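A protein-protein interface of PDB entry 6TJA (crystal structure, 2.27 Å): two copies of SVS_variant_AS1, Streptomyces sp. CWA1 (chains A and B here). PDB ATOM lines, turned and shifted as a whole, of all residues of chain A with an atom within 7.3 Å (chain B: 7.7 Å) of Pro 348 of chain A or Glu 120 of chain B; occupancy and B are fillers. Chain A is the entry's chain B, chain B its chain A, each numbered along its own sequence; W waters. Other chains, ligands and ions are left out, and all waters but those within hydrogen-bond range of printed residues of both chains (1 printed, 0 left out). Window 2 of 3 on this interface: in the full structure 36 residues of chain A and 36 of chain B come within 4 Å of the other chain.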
ATOM      1  N   LEU A 175       9.116  33.309   5.428  1.00  0.00           N
ATOM      2  CA  LEU A 175       8.041  32.283   5.471  1.00  0.00           C
ATOM      3  C   LEU A 175       8.453  31.078   4.620  1.00  0.00           C
ATOM      4  O   LEU A 175       8.391  29.945   5.130  1.00  0.00           O
ATOM      5  CB  LEU A 175       6.722  32.897   4.986  1.00  0.00           C
ATOM      6  CG  LEU A 175       5.512  31.962   5.025  1.00  0.00           C
ATOM      7  CD1 LEU A 175       5.271  31.433   6.434  1.00  0.00           C
ATOM      8  CD2 LEU A 175       4.266  32.656   4.494  1.00  0.00           C
ATOM      9  N   ASP A 176       8.883  31.302   3.387  1.00  0.00           N
ATOM     10  CA  ASP A 176       9.165  30.207   2.423  1.00  0.00           C
ATOM     11  C   ASP A 176      10.251  29.278   3.016  1.00  0.00           C
ATOM     12  O   ASP A 176      10.005  28.079   3.143  1.00  0.00           O
ATOM     13  CB  ASP A 176       9.592  30.759   1.066  1.00  0.00           C
ATOM     14  CG  ASP A 176       9.610  29.705  -0.039  1.00  0.00           C
ATOM     15  OD1 ASP A 176       8.532  29.087  -0.298  1.00  0.00           O
ATOM     16  OD2 ASP A 176      10.688  29.514  -0.641  1.00  0.00           O
ATOM     17  N   ASP A 177      11.407  29.827   3.392  1.00  0.00           N
ATOM     18  CA  ASP A 177      12.543  29.065   3.966  1.00  0.00           C
ATOM     19  C   ASP A 177      12.078  28.379   5.256  1.00  0.00           C
ATOM     20  O   ASP A 177      12.349  27.177   5.398  1.00  0.00           O
ATOM     21  CB  ASP A 177      13.769  29.956   4.211  1.00  0.00           C
ATOM     22  CG  ASP A 177      14.588  30.305   2.979  1.00  0.00           C
ATOM     23  OD1 ASP A 177      14.413  29.661   1.949  1.00  0.00           O
ATOM     24  OD2 ASP A 177      15.420  31.217   3.076  1.00  0.00           O
ATOM     25  N   PRO A 343      -2.904  28.813  -3.519  1.00  0.00           N
ATOM     26  CA  PRO A 343      -1.611  28.649  -2.857  1.00  0.00           C
ATOM     27  C   PRO A 343      -1.291  29.832  -1.916  1.00  0.00           C
ATOM     28  O   PRO A 343      -1.631  30.940  -2.248  1.00  0.00           O
ATOM     29  CB  PRO A 343      -0.591  28.582  -4.008  1.00  0.00           C
ATOM     30  CG  PRO A 343      -1.409  28.419  -5.293  1.00  0.00           C
ATOM     31  CD  PRO A 343      -2.807  28.912  -4.984  1.00  0.00           C
ATOM     32  N   LEU A 344      -0.676  29.564  -0.758  1.00  0.00           N
ATOM     33  CA  LEU A 344      -0.083  30.593   0.131  1.00  0.00           C
ATOM     34  C   LEU A 344       0.783  31.534  -0.700  1.00  0.00           C
ATOM     35  O   LEU A 344       1.732  31.087  -1.342  1.00  0.00           O
ATOM     36  CB  LEU A 344       0.775  29.916   1.204  1.00  0.00           C
ATOM     37  CG  LEU A 344       0.020  29.183   2.306  1.00  0.00           C
ATOM     38  CD1 LEU A 344       0.932  28.927   3.496  1.00  0.00           C
ATOM     39  CD2 LEU A 344      -1.205  29.973   2.744  1.00  0.00           C
ATOM     40  N   PRO A 345       0.508  32.860  -0.712  1.00  0.00           N
ATOM     41  CA  PRO A 345       1.458  33.813  -1.277  1.00  0.00           C
ATOM     42  C   PRO A 345       2.600  33.934  -0.255  1.00  0.00           C
ATOM     43  O   PRO A 345       2.327  33.843   0.943  1.00  0.00           O
ATOM     44  CB  PRO A 345       0.644  35.104  -1.496  1.00  0.00           C
ATOM     45  CG  PRO A 345      -0.791  34.745  -1.111  1.00  0.00           C
ATOM     46  CD  PRO A 345      -0.701  33.532  -0.203  1.00  0.00           C
ATOM     47  N   GLY A 346       3.833  34.055  -0.753  1.00  0.00           N
ATOM     48  CA  GLY A 346       5.067  34.153   0.054  1.00  0.00           C
ATOM     49  C   GLY A 346       5.752  32.802   0.262  1.00  0.00           C
ATOM     50  O   GLY A 346       6.850  32.803   0.850  1.00  0.00           O
ATOM     51  N   ALA A 347       5.141  31.698  -0.208  1.00  0.00           N
ATOM     52  CA  ALA A 347       5.548  30.296   0.062  1.00  0.00           C
ATOM     53  C   ALA A 347       5.584  29.507  -1.245  1.00  0.00           C
ATOM     54  O   ALA A 347       5.027  28.429  -1.378  1.00  0.00           O
ATOM     55  CB  ALA A 347       4.627  29.699   1.089  1.00  0.00           C
ATOM     56  N   PRO A 348       6.336  29.992  -2.246  1.00  0.00           N
ATOM     57  CA  PRO A 348       6.433  29.285  -3.519  1.00  0.00           C
ATOM     58  C   PRO A 348       7.011  27.858  -3.436  1.00  0.00           C
ATOM     59  O   PRO A 348       6.725  27.135  -4.354  1.00  0.00           O
ATOM     60  CB  PRO A 348       7.300  30.226  -4.361  1.00  0.00           C
ATOM     61  CG  PRO A 348       8.110  31.023  -3.339  1.00  0.00           C
ATOM     62  CD  PRO A 348       7.158  31.215  -2.183  1.00  0.00           C
ATOM     63  N   SER A 349       7.718  27.446  -2.358  1.00  0.00           N
ATOM     64  CA  SER A 349       8.289  26.070  -2.224  1.00  0.00           C
ATOM     65  C   SER A 349       7.174  25.034  -2.010  1.00  0.00           C
ATOM     66  O   SER A 349       7.425  23.849  -2.248  1.00  0.00           O
ATOM     67  CB  SER A 349       9.347  25.970  -1.144  1.00  0.00           C
ATOM     68  OG  SER A 349       8.774  26.104   0.156  1.00  0.00           O
ATOM     69  N   ILE A 350       5.978  25.446  -1.584  1.00  0.00           N
ATOM     70  CA  ILE A 350       4.847  24.509  -1.321  1.00  0.00           C
ATOM     71  C   ILE A 350       3.684  24.736  -2.314  1.00  0.00           C
ATOM     72  O   ILE A 350       2.711  23.996  -2.202  1.00  0.00           O
ATOM     73  CB  ILE A 350       4.376  24.622   0.140  1.00  0.00           C
ATOM     74  CG1 ILE A 350       3.627  25.941   0.383  1.00  0.00           C
ATOM     75  CG2 ILE A 350       5.553  24.419   1.088  1.00  0.00           C
ATOM     76  CD1 ILE A 350       2.929  26.036   1.705  1.00  0.00           C
ATOM     77  N   ALA A 351       3.773  25.677  -3.264  1.00  0.00           N
ATOM     78  CA  ALA A 351       2.650  26.034  -4.182  1.00  0.00           C
ATOM     79  C   ALA A 351       2.293  24.850  -5.094  1.00  0.00           C
ATOM     80  O   ALA A 351       1.125  24.746  -5.496  1.00  0.00           O
ATOM     81  CB  ALA A 351       2.993  27.264  -4.982  1.00  0.00           C
ATOM     82  N   TRP A 352       3.248  23.964  -5.397  1.00  0.00           N
ATOM     83  CA  TRP A 352       2.978  22.775  -6.240  1.00  0.00           C
ATOM     84  C   TRP A 352       1.931  21.887  -5.566  1.00  0.00           C
ATOM     85  O   TRP A 352       1.284  21.114  -6.259  1.00  0.00           O
ATOM     86  CB  TRP A 352       4.272  22.027  -6.572  1.00  0.00           C
ATOM     87  CG  TRP A 352       4.953  21.347  -5.428  1.00  0.00           C
ATOM     88  CD1 TRP A 352       5.868  21.879  -4.569  1.00  0.00           C
ATOM     89  CD2 TRP A 352       4.826  19.971  -5.063  1.00  0.00           C
ATOM     90  NE1 TRP A 352       6.297  20.938  -3.670  1.00  0.00           N
ATOM     91  CE2 TRP A 352       5.682  19.752  -3.951  1.00  0.00           C
ATOM     92  CE3 TRP A 352       4.070  18.907  -5.555  1.00  0.00           C
ATOM     93  CZ2 TRP A 352       5.798  18.510  -3.326  1.00  0.00           C
ATOM     94  CZ3 TRP A 352       4.189  17.676  -4.941  1.00  0.00           C
ATOM     95  CH2 TRP A 352       5.037  17.483  -3.840  1.00  0.00           C
ATOM     96  N   TRP A 353       1.736  21.999  -4.257  1.00  0.00           N
ATOM     97  CA  TRP A 353       0.677  21.209  -3.575  1.00  0.00           C
ATOM     98  C   TRP A 353      -0.702  21.517  -4.189  1.00  0.00           C
ATOM     99  O   TRP A 353      -1.574  20.678  -4.032  1.00  0.00           O
ATOM    100  CB  TRP A 353       0.641  21.476  -2.076  1.00  0.00           C
ATOM    101  CG  TRP A 353       1.840  21.067  -1.279  1.00  0.00           C
ATOM    102  CD1 TRP A 353       2.871  20.255  -1.652  1.00  0.00           C
ATOM    103  CD2 TRP A 353       2.110  21.467   0.077  1.00  0.00           C
ATOM    104  NE1 TRP A 353       3.758  20.125  -0.622  1.00  0.00           N
ATOM    105  CE2 TRP A 353       3.340  20.885   0.440  1.00  0.00           C
ATOM    106  CE3 TRP A 353       1.464  22.304   0.989  1.00  0.00           C
ATOM    107  CZ2 TRP A 353       3.902  21.069   1.701  1.00  0.00           C
ATOM    108  CZ3 TRP A 353       2.021  22.490   2.244  1.00  0.00           C
ATOM    109  CH2 TRP A 353       3.219  21.867   2.597  1.00  0.00           C
ATOM    110  N   ARG B 109      17.976  24.893   0.732  1.00  0.00           N
ATOM    111  CA  ARG B 109      17.304  25.657  -0.362  1.00  0.00           C
ATOM    112  C   ARG B 109      17.476  24.887  -1.683  1.00  0.00           C
ATOM    113  O   ARG B 109      16.490  24.712  -2.380  1.00  0.00           O
ATOM    114  CB  ARG B 109      17.787  27.109  -0.451  1.00  0.00           C
ATOM    115  CG  ARG B 109      17.355  28.002   0.716  1.00  0.00           C
ATOM    116  CD  ARG B 109      17.583  29.507   0.581  1.00  0.00           C
ATOM    117  NE  ARG B 109      18.864  29.776  -0.041  1.00  0.00           N
ATOM    118  CZ  ARG B 109      20.016  30.031   0.606  1.00  0.00           C
ATOM    119  NH1 ARG B 109      20.058  30.094   1.932  1.00  0.00           N
ATOM    120  NH2 ARG B 109      21.128  30.237  -0.093  1.00  0.00           N
ATOM    121  N   ARG B 112      15.403  21.608  -1.704  1.00  0.00           N
ATOM    122  CA  ARG B 112      13.961  21.925  -1.841  1.00  0.00           C
ATOM    123  C   ARG B 112      13.623  22.256  -3.303  1.00  0.00           C
ATOM    124  O   ARG B 112      12.626  21.718  -3.803  1.00  0.00           O
ATOM    125  CB  ARG B 112      13.538  23.040  -0.886  1.00  0.00           C
ATOM    126  CG  ARG B 112      12.036  23.313  -0.908  1.00  0.00           C
ATOM    127  CD  ARG B 112      11.251  22.127  -0.385  1.00  0.00           C
ATOM    128  NE  ARG B 112       9.822  22.196  -0.615  1.00  0.00           N
ATOM    129  CZ  ARG B 112       8.992  21.158  -0.551  1.00  0.00           C
ATOM    130  NH1 ARG B 112       9.452  19.952  -0.252  1.00  0.00           N
ATOM    131  NH2 ARG B 112       7.691  21.338  -0.742  1.00  0.00           N
ATOM    132  N   ALA B 113      14.451  23.044  -3.979  1.00  0.00           N
ATOM    133  CA  ALA B 113      14.307  23.406  -5.412  1.00  0.00           C
ATOM    134  C   ALA B 113      14.247  22.157  -6.294  1.00  0.00           C
ATOM    135  O   ALA B 113      13.488  22.166  -7.301  1.00  0.00           O
ATOM    136  CB  ALA B 113      15.451  24.297  -5.824  1.00  0.00           C
ATOM    137  N   ALA B 116      10.711  20.547  -5.461  1.00  0.00           N
ATOM    138  CA  ALA B 116       9.583  21.407  -5.704  1.00  0.00           C
ATOM    139  C   ALA B 116       9.826  22.354  -6.847  1.00  0.00           C
ATOM    140  O   ALA B 116      10.569  23.259  -6.724  1.00  0.00           O
ATOM    141  CB  ALA B 116       9.287  22.183  -4.454  1.00  0.00           C
ATOM    142  N   PRO B 117       9.164  22.136  -7.960  1.00  0.00           N
ATOM    143  CA  PRO B 117       9.268  22.942  -9.171  1.00  0.00           C
ATOM    144  C   PRO B 117       8.783  24.361  -8.993  1.00  0.00           C
ATOM    145  O   PRO B 117       9.229  25.203  -9.703  1.00  0.00           O
ATOM    146  CB  PRO B 117       8.398  22.198 -10.173  1.00  0.00           C
ATOM    147  CG  PRO B 117       8.224  20.871  -9.627  1.00  0.00           C
ATOM    148  CD  PRO B 117       8.302  20.976  -8.149  1.00  0.00           C
ATOM    149  N   SER B 118       7.902  24.599  -8.042  1.00  0.00           N
ATOM    150  CA  SER B 118       7.372  25.963  -7.763  1.00  0.00           C
ATOM    151  C   SER B 118       8.405  26.801  -6.988  1.00  0.00           C
ATOM    152  O   SER B 118       8.273  28.038  -6.945  1.00  0.00           O
ATOM    153  CB  SER B 118       6.044  25.905  -7.049  1.00  0.00           C
ATOM    154  OG  SER B 118       6.112  25.113  -5.870  1.00  0.00           O
ATOM    155  N   ALA B 119       9.425  26.161  -6.429  1.00  0.00           N
ATOM    156  CA  ALA B 119      10.507  26.830  -5.682  1.00  0.00           C
ATOM    157  C   ALA B 119      11.106  27.951  -6.545  1.00  0.00           C
ATOM    158  O   ALA B 119      11.253  27.737  -7.784  1.00  0.00           O
ATOM    159  CB  ALA B 119      11.555  25.818  -5.273  1.00  0.00           C
ATOM    160  N   GLU B 120      11.452  29.050  -5.893  1.00  0.00           N
ATOM    161  CA  GLU B 120      12.066  30.215  -6.477  1.00  0.00           C
ATOM    162  C   GLU B 120      13.532  30.232  -6.103  1.00  0.00           C
ATOM    163  O   GLU B 120      13.896  29.715  -5.104  1.00  0.00           O
ATOM    164  CB  GLU B 120      11.333  31.474  -6.038  1.00  0.00           C
ATOM    165  CG  GLU B 120      10.346  31.931  -7.095  1.00  0.00           C
ATOM    166  CD  GLU B 120       9.239  32.784  -6.562  1.00  0.00           C
ATOM    167  OE1 GLU B 120       9.511  33.618  -5.704  1.00  0.00           O
ATOM    168  OE2 GLU B 120       8.099  32.633  -7.015  1.00  0.00           O
ATOM    169  N   ASP B 121      14.372  30.769  -6.955  1.00  0.00           N
ATOM    170  CA  ASP B 121      15.803  30.780  -6.756  1.00  0.00           C
ATOM    171  C   ASP B 121      16.466  31.561  -5.652  1.00  0.00           C
ATOM    172  O   ASP B 121      17.457  31.123  -5.125  1.00  0.00           O
ATOM    173  CB  ASP B 121      16.541  30.997  -8.073  1.00  0.00           C
ATOM    174  CG  ASP B 121      16.568  32.417  -8.510  1.00  0.00           C
ATOM    175  OD1 ASP B 121      16.285  32.684  -9.664  1.00  0.00           O
ATOM    176  OD2 ASP B 121      16.855  33.284  -7.693  1.00  0.00           O
ATOM    177  N   ASN B 122      15.928  32.736  -5.361  1.00  0.00           N
ATOM    178  CA  ASN B 122      16.473  33.715  -4.439  1.00  0.00           C
ATOM    179  C   ASN B 122      17.957  34.100  -4.635  1.00  0.00           C
ATOM    180  O   ASN B 122      18.780  33.949  -3.765  1.00  0.00           O
ATOM    181  CB  ASN B 122      15.997  33.563  -2.983  1.00  0.00           C
ATOM    182  CG  ASN B 122      16.543  32.357  -2.299  1.00  0.00           C
ATOM    183  OD1 ASN B 122      17.729  32.152  -2.279  1.00  0.00           O
ATOM    184  ND2 ASN B 122      15.671  31.561  -1.711  1.00  0.00           N
ATOM    185  N   GLY B 123      18.248  34.604  -5.821  1.00  0.00           N
ATOM    186  CA  GLY B 123      19.547  35.114  -6.212  1.00  0.00           C
ATOM    187  C   GLY B 123      20.579  34.025  -6.436  1.00  0.00           C
ATOM    188  O   GLY B 123      21.774  34.315  -6.511  1.00  0.00           O
ATOM    189  N   ASP B 124      20.137  32.774  -6.544  1.00  0.00           N
ATOM    190  CA  ASP B 124      21.067  31.702  -6.757  1.00  0.00           C
ATOM    191  C   ASP B 124      21.102  31.220  -8.184  1.00  0.00           C
ATOM    192  O   ASP B 124      20.146  30.683  -8.659  1.00  0.00           O
ATOM    193  CB  ASP B 124      20.581  30.620  -5.903  1.00  0.00           C
ATOM    194  CG  ASP B 124      21.603  29.761  -5.540  1.00  0.00           C
ATOM    195  OD1 ASP B 124      22.478  29.510  -6.369  1.00  0.00           O
ATOM    196  OD2 ASP B 124      21.712  29.390  -4.386  1.00  0.00           O
ATOM    197  N   VAL B 127      20.401  27.380  -9.000  1.00  0.00           N
ATOM    198  CA  VAL B 127      19.071  26.766  -8.716  1.00  0.00           C
ATOM    199  C   VAL B 127      18.279  26.594 -10.013  1.00  0.00           C
ATOM    200  O   VAL B 127      17.826  25.482 -10.264  1.00  0.00           O
ATOM    201  CB  VAL B 127      18.297  27.488  -7.600  1.00  0.00           C
ATOM    202  CG1 VAL B 127      16.792  27.282  -7.695  1.00  0.00           C
ATOM    203  CG2 VAL B 127      18.824  27.059  -6.243  1.00  0.00           C
ATOM    204  N   PRO B 128      18.076  27.620 -10.873  1.00  0.00           N
ATOM    205  CA  PRO B 128      17.291  27.441 -12.098  1.00  0.00           C
ATOM    206  C   PRO B 128      17.868  26.338 -13.006  1.00  0.00           C
ATOM    207  O   PRO B 128      17.105  25.531 -13.498  1.00  0.00           O
ATOM    208  CB  PRO B 128      17.322  28.820 -12.803  1.00  0.00           C
ATOM    209  CG  PRO B 128      17.650  29.792 -11.665  1.00  0.00           C
ATOM    210  CD  PRO B 128      18.539  29.011 -10.716  1.00  0.00           C
ATOM    211  N   GLN B 131      16.876  23.055 -11.665  1.00  0.00           N
ATOM    212  CA  GLN B 131      15.412  22.857 -11.842  1.00  0.00           C
ATOM    213  C   GLN B 131      15.117  22.400 -13.275  1.00  0.00           C
ATOM    214  O   GLN B 131      14.127  21.649 -13.457  1.00  0.00           O
ATOM    215  CB  GLN B 131      14.646  24.118 -11.456  1.00  0.00           C
ATOM    216  CG  GLN B 131      14.544  24.301  -9.949  1.00  0.00           C
ATOM    217  CD  GLN B 131      13.639  25.450  -9.594  1.00  0.00           C
ATOM    218  OE1 GLN B 131      13.829  26.550 -10.085  1.00  0.00           O
ATOM    219  NE2 GLN B 131      12.665  25.200  -8.731  1.00  0.00           N
HETATM  220  O   HOH W   1      11.390  28.845  -2.911  1.00  0.00           O
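N of Trp 352 of chain A is in hydrogen-bond range of OG of Ser 118 of chain B, at 3.1 Å. NE1 of Trp 352 of chain A lies close to NH2 of Arg 112 of chain B (3.3 Å). The backbone carbonyl oxygen of Pro 348 of chain A lies within hydrogen-bond range of the side-chain hydroxyl of Ser 118 of chain B (2.6 Å). The guanidinium group of Arg 112 of chain B is in hydrogen-bond range of the backbone carbonyl oxygen of Ser 349 of chain A (2.9 Å).
O of Ala 116 of chain B lies within hydrogen-bond range of NE2 of Gln 131 of chain B (3.5 Å). The backbone NH of Ser 349 of chain A is in hydrogen-bond range of the side-chain carboxylate of Asp 176 of chain A, at 2.8 Å. The side-chain amide oxygen (OD1) of Asn 122 of chain B sits at hydrogen-bond distance from the guanidinium group (NE) of Arg 109 of chain B (3.5 Å). O of Ala 119 of chain B sits at hydrogen-bond distance from NE2 of Gln 131 of chain B, at 3.1 Å. The indole nitrogen (NE1) of Trp 352 of chain A sits close to the backbone carbonyl oxygen (O) of Ser 349 of chain A, 3.4 Å away.
CD of Arg 109 of chain B touches OD1 of Asp 177 of chain A, at 3.5 Å. Pro 348 of chain A touches Ala 119 of chain B (O to N, 3.5 Å). Pro 348 of chain A touches Glu 120 of chain B. Ala 116 of chain B touches Ser 349 of chain A (CB to O, 3.3 Å). Ala 351 of chain A touches Ser 118 of chain B. Trp 352 of chain A touches Ala 116 of chain B (NE1 to CB, 3.3 Å).
Pro 348 of chain A touches just these residues of chain B: Ser 118 (2.6 Å), Ala 119 (3.5 Å) and Glu 120 (3.7 Å). Glu 120 of chain B touches just one residue of chain A: Pro 348. Printed residues of chain A within 4 Å of Ser 118 of chain B: Pro 348, Ala 351 and Trp 352. Of the printed residues of chain B, Trp 352 of chain A touches Arg 112 (3.3 Å), Ala 116 (3.3 Å) and Ser 118 (3.1 Å). Printed residues of chain B within 4 Å of Asp 177 of chain A: Arg 109 (3.5 Å). Printed residues of chain B within 4 Å of Ser 349 of chain A: Arg 112 and Ala 116. Asp 124 of chain B touches none of the printed residues of chain A. The nearest residue of chain B that does not touch Pro 348 of chain A is Ala 116 of chain B (5.6 Å). The nearest printed residue of chain A that does not touch Arg 112 of chain B is Trp 353 of chain A (4.1 Å).
Printed residues of chain A that touch a printed residue of chain B: Asp 177, Pro 348, Ser 349, Ala 351 and Trp 352. Hydrophobic or aromatic side chains of chain A within 4 Å of the printed part of chain B: Pro 348, Ala 351 and Trp 352. Of the 15 printed residues of chain B, 6 touch a printed residue of chain A. Hydrophobic or aromatic side chains of chain B that line the printed part of chain A: Ala 116. Among the printed residues, no Asp or Glu carboxylate lies within 4 Å of a Lys or Arg side-chain nitrogen of the other chain.
No position is printed for both chains. Of the 10 pairs that touch across the chains among the printed residues, none has its exchanged pair printed and touching as well.
Water W1 lies within hydrogen-bond range of OD2 of Asp 176 of chain A (2.5 Å) and N of Glu 120 of chain B (3.0 Å).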
